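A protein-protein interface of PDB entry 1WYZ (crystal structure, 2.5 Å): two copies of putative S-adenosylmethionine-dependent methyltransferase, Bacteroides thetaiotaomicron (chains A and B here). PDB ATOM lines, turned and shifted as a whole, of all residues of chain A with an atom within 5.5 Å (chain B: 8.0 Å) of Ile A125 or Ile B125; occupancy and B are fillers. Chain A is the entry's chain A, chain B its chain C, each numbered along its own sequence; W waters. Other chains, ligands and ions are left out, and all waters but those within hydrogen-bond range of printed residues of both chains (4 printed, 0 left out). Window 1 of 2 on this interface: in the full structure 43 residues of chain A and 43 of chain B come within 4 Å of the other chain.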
ATOM      1  N   GLY A 120      22.848 -15.629  11.007  1.00  0.00           N
ATOM      2  CA  GLY A 120      22.180 -16.123  12.186  1.00  0.00           C
ATOM      3  C   GLY A 120      22.897 -17.326  12.746  1.00  0.00           C
ATOM      4  O   GLY A 120      23.804 -17.865  12.108  1.00  0.00           O
ATOM      5  N   PRO A 121      22.520 -17.771  13.947  1.00  0.00           N
ATOM      6  CA  PRO A 121      23.224 -18.934  14.469  1.00  0.00           C
ATOM      7  C   PRO A 121      22.815 -20.177  13.682  1.00  0.00           C
ATOM      8  O   PRO A 121      21.642 -20.358  13.344  1.00  0.00           O
ATOM      9  CB  PRO A 121      22.772 -18.972  15.925  1.00  0.00           C
ATOM     10  CG  PRO A 121      21.343 -18.547  15.824  1.00  0.00           C
ATOM     11  CD  PRO A 121      21.399 -17.387  14.821  1.00  0.00           C
ATOM     12  N   SER A 122      23.804 -21.003  13.353  1.00  0.00           N
ATOM     13  CA  SER A 122      23.581 -22.259  12.644  1.00  0.00           C
ATOM     14  C   SER A 122      24.299 -23.318  13.457  1.00  0.00           C
ATOM     15  O   SER A 122      25.532 -23.295  13.569  1.00  0.00           O
ATOM     16  CB  SER A 122      24.178 -22.235  11.232  1.00  0.00           C
ATOM     17  OG  SER A 122      24.220 -23.550  10.678  1.00  0.00           O
ATOM     18  N   SER A 123      23.537 -24.235  14.039  1.00  0.00           N
ATOM     19  CA  SER A 123      24.138 -25.291  14.831  1.00  0.00           C
ATOM     20  C   SER A 123      25.038 -26.115  13.922  1.00  0.00           C
ATOM     21  O   SER A 123      25.967 -26.760  14.387  1.00  0.00           O
ATOM     22  CB  SER A 123      23.054 -26.172  15.452  1.00  0.00           C
ATOM     23  OG  SER A 123      22.167 -26.634  14.466  1.00  0.00           O
ATOM     24  N   ILE A 124      24.766 -26.086  12.622  1.00  0.00           N
ATOM     25  CA  ILE A 124      25.588 -26.830  11.687  1.00  0.00           C
ATOM     26  C   ILE A 124      27.009 -26.265  11.561  1.00  0.00           C
ATOM     27  O   ILE A 124      27.966 -27.003  11.793  1.00  0.00           O
ATOM     28  CB  ILE A 124      24.911 -26.918  10.300  1.00  0.00           C
ATOM     29  CG1 ILE A 124      23.795 -27.956  10.346  1.00  0.00           C
ATOM     30  CG2 ILE A 124      25.920 -27.353   9.230  1.00  0.00           C
ATOM     31  CD1 ILE A 124      22.532 -27.509  11.078  1.00  0.00           C
ATOM     32  N   ILE A 125      27.166 -24.978  11.224  1.00  0.00           N
ATOM     33  CA  ILE A 125      28.527 -24.427  11.087  1.00  0.00           C
ATOM     34  C   ILE A 125      29.207 -24.176  12.434  1.00  0.00           C
ATOM     35  O   ILE A 125      30.423 -24.310  12.545  1.00  0.00           O
ATOM     36  CB  ILE A 125      28.583 -23.097  10.275  1.00  0.00           C
ATOM     37  CG1 ILE A 125      28.137 -21.933  11.152  1.00  0.00           C
ATOM     38  CG2 ILE A 125      27.708 -23.195   9.023  1.00  0.00           C
ATOM     39  CD1 ILE A 125      28.538 -20.556  10.644  1.00  0.00           C
ATOM     40  N   LEU A 126      28.432 -23.798  13.449  1.00  0.00           N
ATOM     41  CA  LEU A 126      28.992 -23.571  14.775  1.00  0.00           C
ATOM     42  C   LEU A 126      29.616 -24.880  15.268  1.00  0.00           C
ATOM     43  O   LEU A 126      30.703 -24.878  15.864  1.00  0.00           O
ATOM     44  CB  LEU A 126      27.903 -23.093  15.744  1.00  0.00           C
ATOM     45  CG  LEU A 126      27.507 -21.619  15.558  1.00  0.00           C
ATOM     46  CD1 LEU A 126      26.225 -21.291  16.329  1.00  0.00           C
ATOM     47  CD2 LEU A 126      28.666 -20.718  16.010  1.00  0.00           C
ATOM     48  N   SER A 127      28.935 -25.996  14.999  1.00  0.00           N
ATOM     49  CA  SER A 127      29.426 -27.322  15.399  1.00  0.00           C
ATOM     50  C   SER A 127      30.715 -27.658  14.688  1.00  0.00           C
ATOM     51  O   SER A 127      31.694 -28.039  15.316  1.00  0.00           O
ATOM     52  CB  SER A 127      28.397 -28.414  15.088  1.00  0.00           C
ATOM     53  OG  SER A 127      27.397 -28.444  16.085  1.00  0.00           O
ATOM     54  N   VAL A 128      30.707 -27.541  13.368  1.00  0.00           N
ATOM     55  CA  VAL A 128      31.909 -27.826  12.605  1.00  0.00           C
ATOM     56  C   VAL A 128      33.065 -27.060  13.222  1.00  0.00           C
ATOM     57  O   VAL A 128      34.142 -27.605  13.422  1.00  0.00           O
ATOM     58  CB  VAL A 128      31.756 -27.393  11.135  1.00  0.00           C
ATOM     59  CG1 VAL A 128      33.102 -27.456  10.429  1.00  0.00           C
ATOM     60  CG2 VAL A 128      30.745 -28.306  10.431  1.00  0.00           C
ATOM     61  N   MET A 129      32.816 -25.794  13.538  1.00  0.00           N
ATOM     62  CA  MET A 129      33.829 -24.928  14.111  1.00  0.00           C
ATOM     63  C   MET A 129      34.408 -25.426  15.422  1.00  0.00           C
ATOM     64  O   MET A 129      35.632 -25.499  15.583  1.00  0.00           O
ATOM     65  CB  MET A 129      33.260 -23.518  14.306  1.00  0.00           C
ATOM     66  CG  MET A 129      33.022 -22.725  13.019  1.00  0.00           C
ATOM     67  SD  MET A 129      31.988 -21.099  13.317  1.00  0.00           S
ATOM     68  CE  MET A 129      33.124 -20.284  14.671  1.00  0.00           C
ATOM     69  N   ALA A 130      33.534 -25.782  16.354  1.00  0.00           N
ATOM     70  CA  ALA A 130      33.984 -26.222  17.660  1.00  0.00           C
ATOM     71  C   ALA A 130      34.472 -27.646  17.723  1.00  0.00           C
ATOM     72  O   ALA A 130      35.066 -28.043  18.731  1.00  0.00           O
ATOM     73  CB  ALA A 130      32.881 -26.014  18.690  1.00  0.00           C
ATOM     74  N   PHE A 138      32.119 -30.992   4.539  1.00  0.00           N
ATOM     75  CA  PHE A 138      31.248 -31.631   5.520  1.00  0.00           C
ATOM     76  C   PHE A 138      29.872 -31.812   4.888  1.00  0.00           C
ATOM     77  O   PHE A 138      29.568 -31.175   3.874  1.00  0.00           O
ATOM     78  CB  PHE A 138      31.151 -30.763   6.770  1.00  0.00           C
ATOM     79  CG  PHE A 138      30.608 -29.390   6.505  1.00  0.00           C
ATOM     80  CD1 PHE A 138      29.232 -29.175   6.424  1.00  0.00           C
ATOM     81  CD2 PHE A 138      31.475 -28.304   6.335  1.00  0.00           C
ATOM     82  CE1 PHE A 138      28.724 -27.894   6.180  1.00  0.00           C
ATOM     83  CE2 PHE A 138      30.975 -27.032   6.092  1.00  0.00           C
ATOM     84  CZ  PHE A 138      29.599 -26.822   6.014  1.00  0.00           C
ATOM     85  N   LEU B   7      36.001 -18.842  19.475  1.00  0.00           N
ATOM     86  CA  LEU B   7      36.119 -18.771  18.010  1.00  0.00           C
ATOM     87  C   LEU B   7      35.350 -17.554  17.516  1.00  0.00           C
ATOM     88  O   LEU B   7      34.122 -17.570  17.433  1.00  0.00           O
ATOM     89  CB  LEU B   7      35.549 -20.037  17.376  1.00  0.00           C
ATOM     90  CG  LEU B   7      36.412 -21.304  17.352  1.00  0.00           C
ATOM     91  CD1 LEU B   7      37.207 -21.441  18.625  1.00  0.00           C
ATOM     92  CD2 LEU B   7      35.499 -22.487  17.124  1.00  0.00           C
ATOM     93  N   PRO B   9      34.418 -15.135  14.548  1.00  0.00           N
ATOM     94  CA  PRO B   9      34.437 -14.988  13.091  1.00  0.00           C
ATOM     95  C   PRO B   9      34.540 -13.540  12.608  1.00  0.00           C
ATOM     96  O   PRO B   9      34.157 -12.610  13.316  1.00  0.00           O
ATOM     97  CB  PRO B   9      33.124 -15.640  12.687  1.00  0.00           C
ATOM     98  CG  PRO B   9      32.213 -15.241  13.799  1.00  0.00           C
ATOM     99  CD  PRO B   9      33.064 -15.475  15.033  1.00  0.00           C
ATOM    100  N   PRO B 117      32.109 -21.601  20.195  1.00  0.00           N
ATOM    101  CA  PRO B 117      32.006 -20.904  18.910  1.00  0.00           C
ATOM    102  C   PRO B 117      31.026 -19.734  18.912  1.00  0.00           C
ATOM    103  O   PRO B 117      29.869 -19.901  19.308  1.00  0.00           O
ATOM    104  CB  PRO B 117      31.550 -22.010  17.968  1.00  0.00           C
ATOM    105  CG  PRO B 117      30.575 -22.762  18.854  1.00  0.00           C
ATOM    106  CD  PRO B 117      31.345 -22.864  20.169  1.00  0.00           C
ATOM    107  N   LEU B 118      31.477 -18.557  18.477  1.00  0.00           N
ATOM    108  CA  LEU B 118      30.585 -17.401  18.414  1.00  0.00           C
ATOM    109  C   LEU B 118      29.974 -17.270  17.014  1.00  0.00           C
ATOM    110  O   LEU B 118      30.606 -17.592  16.009  1.00  0.00           O
ATOM    111  CB  LEU B 118      31.324 -16.113  18.809  1.00  0.00           C
ATOM    112  CG  LEU B 118      31.731 -15.981  20.295  1.00  0.00           C
ATOM    113  CD1 LEU B 118      31.788 -14.498  20.689  1.00  0.00           C
ATOM    114  CD2 LEU B 118      30.720 -16.702  21.209  1.00  0.00           C
ATOM    115  N   VAL B 119      28.734 -16.806  16.950  1.00  0.00           N
ATOM    116  CA  VAL B 119      28.026 -16.667  15.678  1.00  0.00           C
ATOM    117  C   VAL B 119      28.666 -15.705  14.706  1.00  0.00           C
ATOM    118  O   VAL B 119      29.221 -14.691  15.106  1.00  0.00           O
ATOM    119  CB  VAL B 119      26.603 -16.188  15.896  1.00  0.00           C
ATOM    120  CG1 VAL B 119      25.950 -15.907  14.577  1.00  0.00           C
ATOM    121  CG2 VAL B 119      25.838 -17.235  16.677  1.00  0.00           C
ATOM    122  N   GLY B 120      28.579 -16.013  13.419  1.00  0.00           N
ATOM    123  CA  GLY B 120      29.155 -15.121  12.433  1.00  0.00           C
ATOM    124  C   GLY B 120      28.667 -15.432  11.039  1.00  0.00           C
ATOM    125  O   GLY B 120      27.861 -16.341  10.857  1.00  0.00           O
ATOM    126  N   PRO B 121      29.128 -14.691  10.024  1.00  0.00           N
ATOM    127  CA  PRO B 121      28.651 -15.003   8.669  1.00  0.00           C
ATOM    128  C   PRO B 121      29.313 -16.270   8.114  1.00  0.00           C
ATOM    129  O   PRO B 121      30.489 -16.517   8.368  1.00  0.00           O
ATOM    130  CB  PRO B 121      28.996 -13.741   7.880  1.00  0.00           C
ATOM    131  CG  PRO B 121      30.262 -13.246   8.583  1.00  0.00           C
ATOM    132  CD  PRO B 121      29.940 -13.459  10.051  1.00  0.00           C
ATOM    133  N   SER B 122      28.530 -17.070   7.392  1.00  0.00           N
ATOM    134  CA  SER B 122      28.968 -18.328   6.773  1.00  0.00           C
ATOM    135  C   SER B 122      28.442 -18.368   5.340  1.00  0.00           C
ATOM    136  O   SER B 122      27.222 -18.329   5.117  1.00  0.00           O
ATOM    137  CB  SER B 122      28.398 -19.524   7.548  1.00  0.00           C
ATOM    138  OG  SER B 122      28.447 -20.713   6.772  1.00  0.00           O
ATOM    139  N   SER B 123      29.338 -18.447   4.364  1.00  0.00           N
ATOM    140  CA  SER B 123      28.870 -18.454   2.980  1.00  0.00           C
ATOM    141  C   SER B 123      28.189 -19.765   2.621  1.00  0.00           C
ATOM    142  O   SER B 123      27.321 -19.793   1.755  1.00  0.00           O
ATOM    143  CB  SER B 123      30.023 -18.162   2.009  1.00  0.00           C
ATOM    144  OG  SER B 123      31.057 -19.105   2.154  1.00  0.00           O
ATOM    145  N   ILE B 124      28.568 -20.846   3.299  1.00  0.00           N
ATOM    146  CA  ILE B 124      27.977 -22.150   3.035  1.00  0.00           C
ATOM    147  C   ILE B 124      26.471 -22.197   3.372  1.00  0.00           C
ATOM    148  O   ILE B 124      25.678 -22.657   2.550  1.00  0.00           O
ATOM    149  CB  ILE B 124      28.681 -23.290   3.841  1.00  0.00           C
ATOM    150  CG1 ILE B 124      30.189 -23.329   3.564  1.00  0.00           C
ATOM    151  CG2 ILE B 124      28.054 -24.632   3.480  1.00  0.00           C
ATOM    152  CD1 ILE B 124      30.637 -23.531   2.092  1.00  0.00           C
ATOM    153  N   ILE B 125      26.069 -21.735   4.560  1.00  0.00           N
ATOM    154  CA  ILE B 125      24.645 -21.792   4.902  1.00  0.00           C
ATOM    155  C   ILE B 125      23.854 -20.629   4.323  1.00  0.00           C
ATOM    156  O   ILE B 125      22.651 -20.754   4.071  1.00  0.00           O
ATOM    157  CB  ILE B 125      24.359 -21.863   6.447  1.00  0.00           C
ATOM    158  CG1 ILE B 125      24.746 -20.559   7.127  1.00  0.00           C
ATOM    159  CG2 ILE B 125      25.095 -23.044   7.066  1.00  0.00           C
ATOM    160  CD1 ILE B 125      24.170 -20.367   8.527  1.00  0.00           C
ATOM    161  N   LEU B 126      24.509 -19.496   4.113  1.00  0.00           N
ATOM    162  CA  LEU B 126      23.800 -18.368   3.532  1.00  0.00           C
ATOM    163  C   LEU B 126      23.388 -18.765   2.103  1.00  0.00           C
ATOM    164  O   LEU B 126      22.322 -18.366   1.614  1.00  0.00           O
ATOM    165  CB  LEU B 126      24.675 -17.097   3.541  1.00  0.00           C
ATOM    166  CG  LEU B 126      24.826 -16.397   4.908  1.00  0.00           C
ATOM    167  CD1 LEU B 126      25.960 -15.363   4.886  1.00  0.00           C
ATOM    168  CD2 LEU B 126      23.513 -15.745   5.285  1.00  0.00           C
ATOM    169  N   SER B 127      24.217 -19.564   1.438  1.00  0.00           N
ATOM    170  CA  SER B 127      23.872 -19.999   0.091  1.00  0.00           C
ATOM    171  C   SER B 127      22.835 -21.127   0.166  1.00  0.00           C
ATOM    172  O   SER B 127      21.965 -21.242  -0.697  1.00  0.00           O
ATOM    173  CB  SER B 127      25.112 -20.460  -0.683  1.00  0.00           C
ATOM    174  OG  SER B 127      25.622 -21.672  -0.180  1.00  0.00           O
ATOM    175  N   VAL B 128      22.915 -21.959   1.199  1.00  0.00           N
ATOM    176  CA  VAL B 128      21.942 -23.028   1.328  1.00  0.00           C
ATOM    177  C   VAL B 128      20.568 -22.401   1.527  1.00  0.00           C
ATOM    178  O   VAL B 128      19.588 -22.878   0.972  1.00  0.00           O
ATOM    179  CB  VAL B 128      22.275 -23.972   2.505  1.00  0.00           C
ATOM    180  CG1 VAL B 128      21.042 -24.767   2.899  1.00  0.00           C
ATOM    181  CG2 VAL B 128      23.373 -24.938   2.088  1.00  0.00           C
ATOM    182  N   MET B 129      20.516 -21.311   2.289  1.00  0.00           N
ATOM    183  CA  MET B 129      19.273 -20.593   2.558  1.00  0.00           C
ATOM    184  C   MET B 129      18.657 -19.891   1.334  1.00  0.00           C
ATOM    185  O   MET B 129      17.437 -19.969   1.093  1.00  0.00           O
ATOM    186  CB  MET B 129      19.503 -19.548   3.654  1.00  0.00           C
ATOM    187  CG  MET B 129      19.833 -20.115   5.024  1.00  0.00           C
ATOM    188  SD  MET B 129      20.511 -18.783   6.295  1.00  0.00           S
ATOM    189  CE  MET B 129      19.062 -17.475   6.267  1.00  0.00           C
ATOM    190  N   ALA B 130      19.482 -19.194   0.557  1.00  0.00           N
ATOM    191  CA  ALA B 130      18.947 -18.476  -0.595  1.00  0.00           C
ATOM    192  C   ALA B 130      18.821 -19.292  -1.884  1.00  0.00           C
ATOM    193  O   ALA B 130      18.273 -18.803  -2.865  1.00  0.00           O
ATOM    194  CB  ALA B 130      19.764 -17.219  -0.843  1.00  0.00           C
ATOM    195  N   SER B 131      19.312 -20.525  -1.876  1.00  0.00           N
ATOM    196  CA  SER B 131      19.258 -21.406  -3.046  1.00  0.00           C
ATOM    197  C   SER B 131      17.875 -21.999  -3.316  1.00  0.00           C
ATOM    198  O   SER B 131      17.537 -22.284  -4.464  1.00  0.00           O
ATOM    199  CB  SER B 131      20.208 -22.573  -2.857  1.00  0.00           C
ATOM    200  OG  SER B 131      19.749 -23.358  -1.764  1.00  0.00           O
ATOM    201  N   PHE B 138      22.413 -31.678   2.723  1.00  0.00           N
ATOM    202  CA  PHE B 138      23.326 -31.112   1.745  1.00  0.00           C
ATOM    203  C   PHE B 138      24.763 -31.487   2.052  1.00  0.00           C
ATOM    204  O   PHE B 138      25.109 -31.794   3.196  1.00  0.00           O
ATOM    205  CB  PHE B 138      23.178 -29.583   1.692  1.00  0.00           C
ATOM    206  CG  PHE B 138      23.523 -28.887   2.980  1.00  0.00           C
ATOM    207  CD1 PHE B 138      24.852 -28.658   3.333  1.00  0.00           C
ATOM    208  CD2 PHE B 138      22.516 -28.462   3.849  1.00  0.00           C
ATOM    209  CE1 PHE B 138      25.178 -28.020   4.537  1.00  0.00           C
ATOM    210  CE2 PHE B 138      22.831 -27.820   5.062  1.00  0.00           C
ATOM    211  CZ  PHE B 138      24.161 -27.601   5.397  1.00  0.00           C
ATOM    212  N   LEU B 170      27.116 -28.982  -3.052  1.00  0.00           N
ATOM    213  CA  LEU B 170      27.728 -27.652  -3.131  1.00  0.00           C
ATOM    214  C   LEU B 170      29.224 -27.789  -3.306  1.00  0.00           C
ATOM    215  O   LEU B 170      29.808 -28.791  -2.911  1.00  0.00           O
ATOM    216  CB  LEU B 170      27.528 -26.846  -1.836  1.00  0.00           C
ATOM    217  CG  LEU B 170      26.238 -26.765  -1.029  1.00  0.00           C
ATOM    218  CD1 LEU B 170      25.877 -28.108  -0.396  1.00  0.00           C
ATOM    219  CD2 LEU B 170      26.449 -25.712   0.055  1.00  0.00           C
ATOM    220  N   ILE B 201      28.219 -12.917  -1.390  1.00  0.00           N
ATOM    221  CA  ILE B 201      27.366 -13.087  -0.219  1.00  0.00           C
ATOM    222  C   ILE B 201      27.650 -12.031   0.859  1.00  0.00           C
ATOM    223  O   ILE B 201      28.796 -11.862   1.301  1.00  0.00           O
ATOM    224  CB  ILE B 201      27.533 -14.499   0.361  1.00  0.00           C
ATOM    225  CG1 ILE B 201      27.483 -15.523  -0.781  1.00  0.00           C
ATOM    226  CG2 ILE B 201      26.405 -14.797   1.345  1.00  0.00           C
ATOM    227  CD1 ILE B 201      27.999 -16.916  -0.419  1.00  0.00           C
ATOM    228  N   ILE B 229      29.825 -19.650  -4.670  1.00  0.00           N
ATOM    229  CA  ILE B 229      29.486 -21.010  -4.322  1.00  0.00           C
ATOM    230  C   ILE B 229      28.484 -21.592  -5.297  1.00  0.00           C
ATOM    231  O   ILE B 229      27.513 -20.943  -5.665  1.00  0.00           O
ATOM    232  CB  ILE B 229      28.949 -21.062  -2.885  1.00  0.00           C
ATOM    233  CG1 ILE B 229      30.137 -20.928  -1.922  1.00  0.00           C
ATOM    234  CG2 ILE B 229      28.142 -22.336  -2.662  1.00  0.00           C
ATOM    235  CD1 ILE B 229      30.701 -19.514  -1.787  1.00  0.00           C
ATOM    236  N   LEU B 231      25.752 -24.651  -6.277  1.00  0.00           N
ATOM    237  CA  LEU B 231      24.870 -25.654  -5.704  1.00  0.00           C
ATOM    238  C   LEU B 231      24.042 -26.361  -6.765  1.00  0.00           C
ATOM    239  O   LEU B 231      23.433 -25.725  -7.632  1.00  0.00           O
ATOM    240  CB  LEU B 231      23.915 -25.020  -4.698  1.00  0.00           C
ATOM    241  CG  LEU B 231      24.522 -24.203  -3.570  1.00  0.00           C
ATOM    242  CD1 LEU B 231      24.905 -22.819  -4.097  1.00  0.00           C
ATOM    243  CD2 LEU B 231      23.511 -24.072  -2.440  1.00  0.00           C
HETATM  244  O   HOH W   1      26.220 -18.501  10.579  1.00  0.00           O
HETATM  245  O   HOH W   2      29.425 -18.922  13.008  1.00  0.00           O
HETATM  246  O   HOH W   3      31.346 -18.543  10.879  1.00  0.00           O
HETATM  247  O   HOH W   4      22.557 -17.407   8.694  1.00  0.00           O
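N of Ile A124 lies close to OG of Ser A122, at 3.2 Å.
OG of Ser A122 is in hydrogen-bond range of N of Ile A125, at 3.3 Å.
The backbone carbonyl oxygen of Leu B7 is in hydrogen-bond range of the backbone NH of Leu B118, 3.0 Å away.
OG of Ser B122 lies close to N of Ile B124 (3.5 Å).
OG of Ser B122 is in hydrogen-bond range of N of Ile B125, at 3.4 Å.
The side-chain hydroxyl (OG) of Ser B127 lies within hydrogen-bond range of the backbone carbonyl oxygen (O) of Ile B124, 2.9 Å away.
Gly A120 touches Val B119.
CG2 of Val B119 touches CB of Pro A121, 3.6 Å away.
Ser A122 touches Ile B125 (CB to CD1, 3.3 Å).
Ile A125 touches Ile B125 (CG2 to CG2, 3.3 Å).
Leu A126 touches Pro B117 (CD2 to O, 3.6 Å).
CD2 of Leu A126 touches O of Leu B118, 3.7 Å away.
Met A129 touches Leu B118.
N of Ala A130 touches CD2 of Leu B7 (3.9 Å).
Pro B117 touches Ala A130 (CD to CB, 3.8 Å).
Ile B124 touches Phe A138.
Printed residues of chain B within 4 Å of Ile A125: Ser B122 (3.3 Å) and Ile B125 (3.3 Å).
Of the printed residues of chain A, Leu B7 touches Met A129 and Ala A130.
Printed residues of chain A within 4 Å of Pro B117: Leu A126 and Ala A130.
Ile B125 touches just these residues of chain A: Ser A122 and Ile A125.
Ala B130 touches none of the printed residues of chain A.
The nearest residue of chain B that does not touch Ile A125 is Gly B120 (4.3 Å).
The nearest residue of chain A that does not touch Ile B125 is Gly A120 (4.4 Å).
The nearest printed residue of chain B that does not touch Pro A121 is Ile B125 (5.3 Å).
Hydrophobic or aromatic side chains of chain A that line the printed part of chain B: Pro A121, Ile A125, Leu A126, Met A129, Ala A130 and Phe A138.
Printed residues of chain B that touch a printed residue of chain A: Leu B7, Pro B117, Leu B118, Val B119, Ser B122, Ile B124, Ile B125 and Phe B138.
Hydrophobic or aromatic side chains of chain B within 4 Å of the printed part of chain A: Leu B7, Pro B117, Val B119, Ile B124, Ile B125 and Phe B138.
Ser A122 touches Ile B125, and with the chains exchanged Ile A125 touches Ser B122.
Ile A125 touches its own counterpart, Ile B125.
Phe A138 touches Ile B124, but with the chains exchanged Ile A124 does not touch Phe B138 (4.2 Å).
Phe A138 touches its own counterpart, Phe B138.
Of the 13 pairs that touch across the chains among the printed residues, 4 have their exchanged pair printed and touching as well.
Water W1 bridges the backbone carbonyl oxygen (O) of Gly B120 (2.7 Å) and the backbone carbonyl oxygen (O) of Gly A120 (2.9 Å).
Water W4 bridges N of Gly A120 (2.9 Å) and SD of Met B129 (3.4 Å).
Water W2 lies within hydrogen-bond range of the backbone NH of Gly B120, the side-chain sulfur of Met A129 and the backbone carbonyl oxygen of Leu B118.
Water W3 lies within hydrogen-bond range of the backbone carbonyl oxygen (O) of Pro B121 (3.3 Å) and the side-chain sulfur (SD) of Met A129 (3.6 Å).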
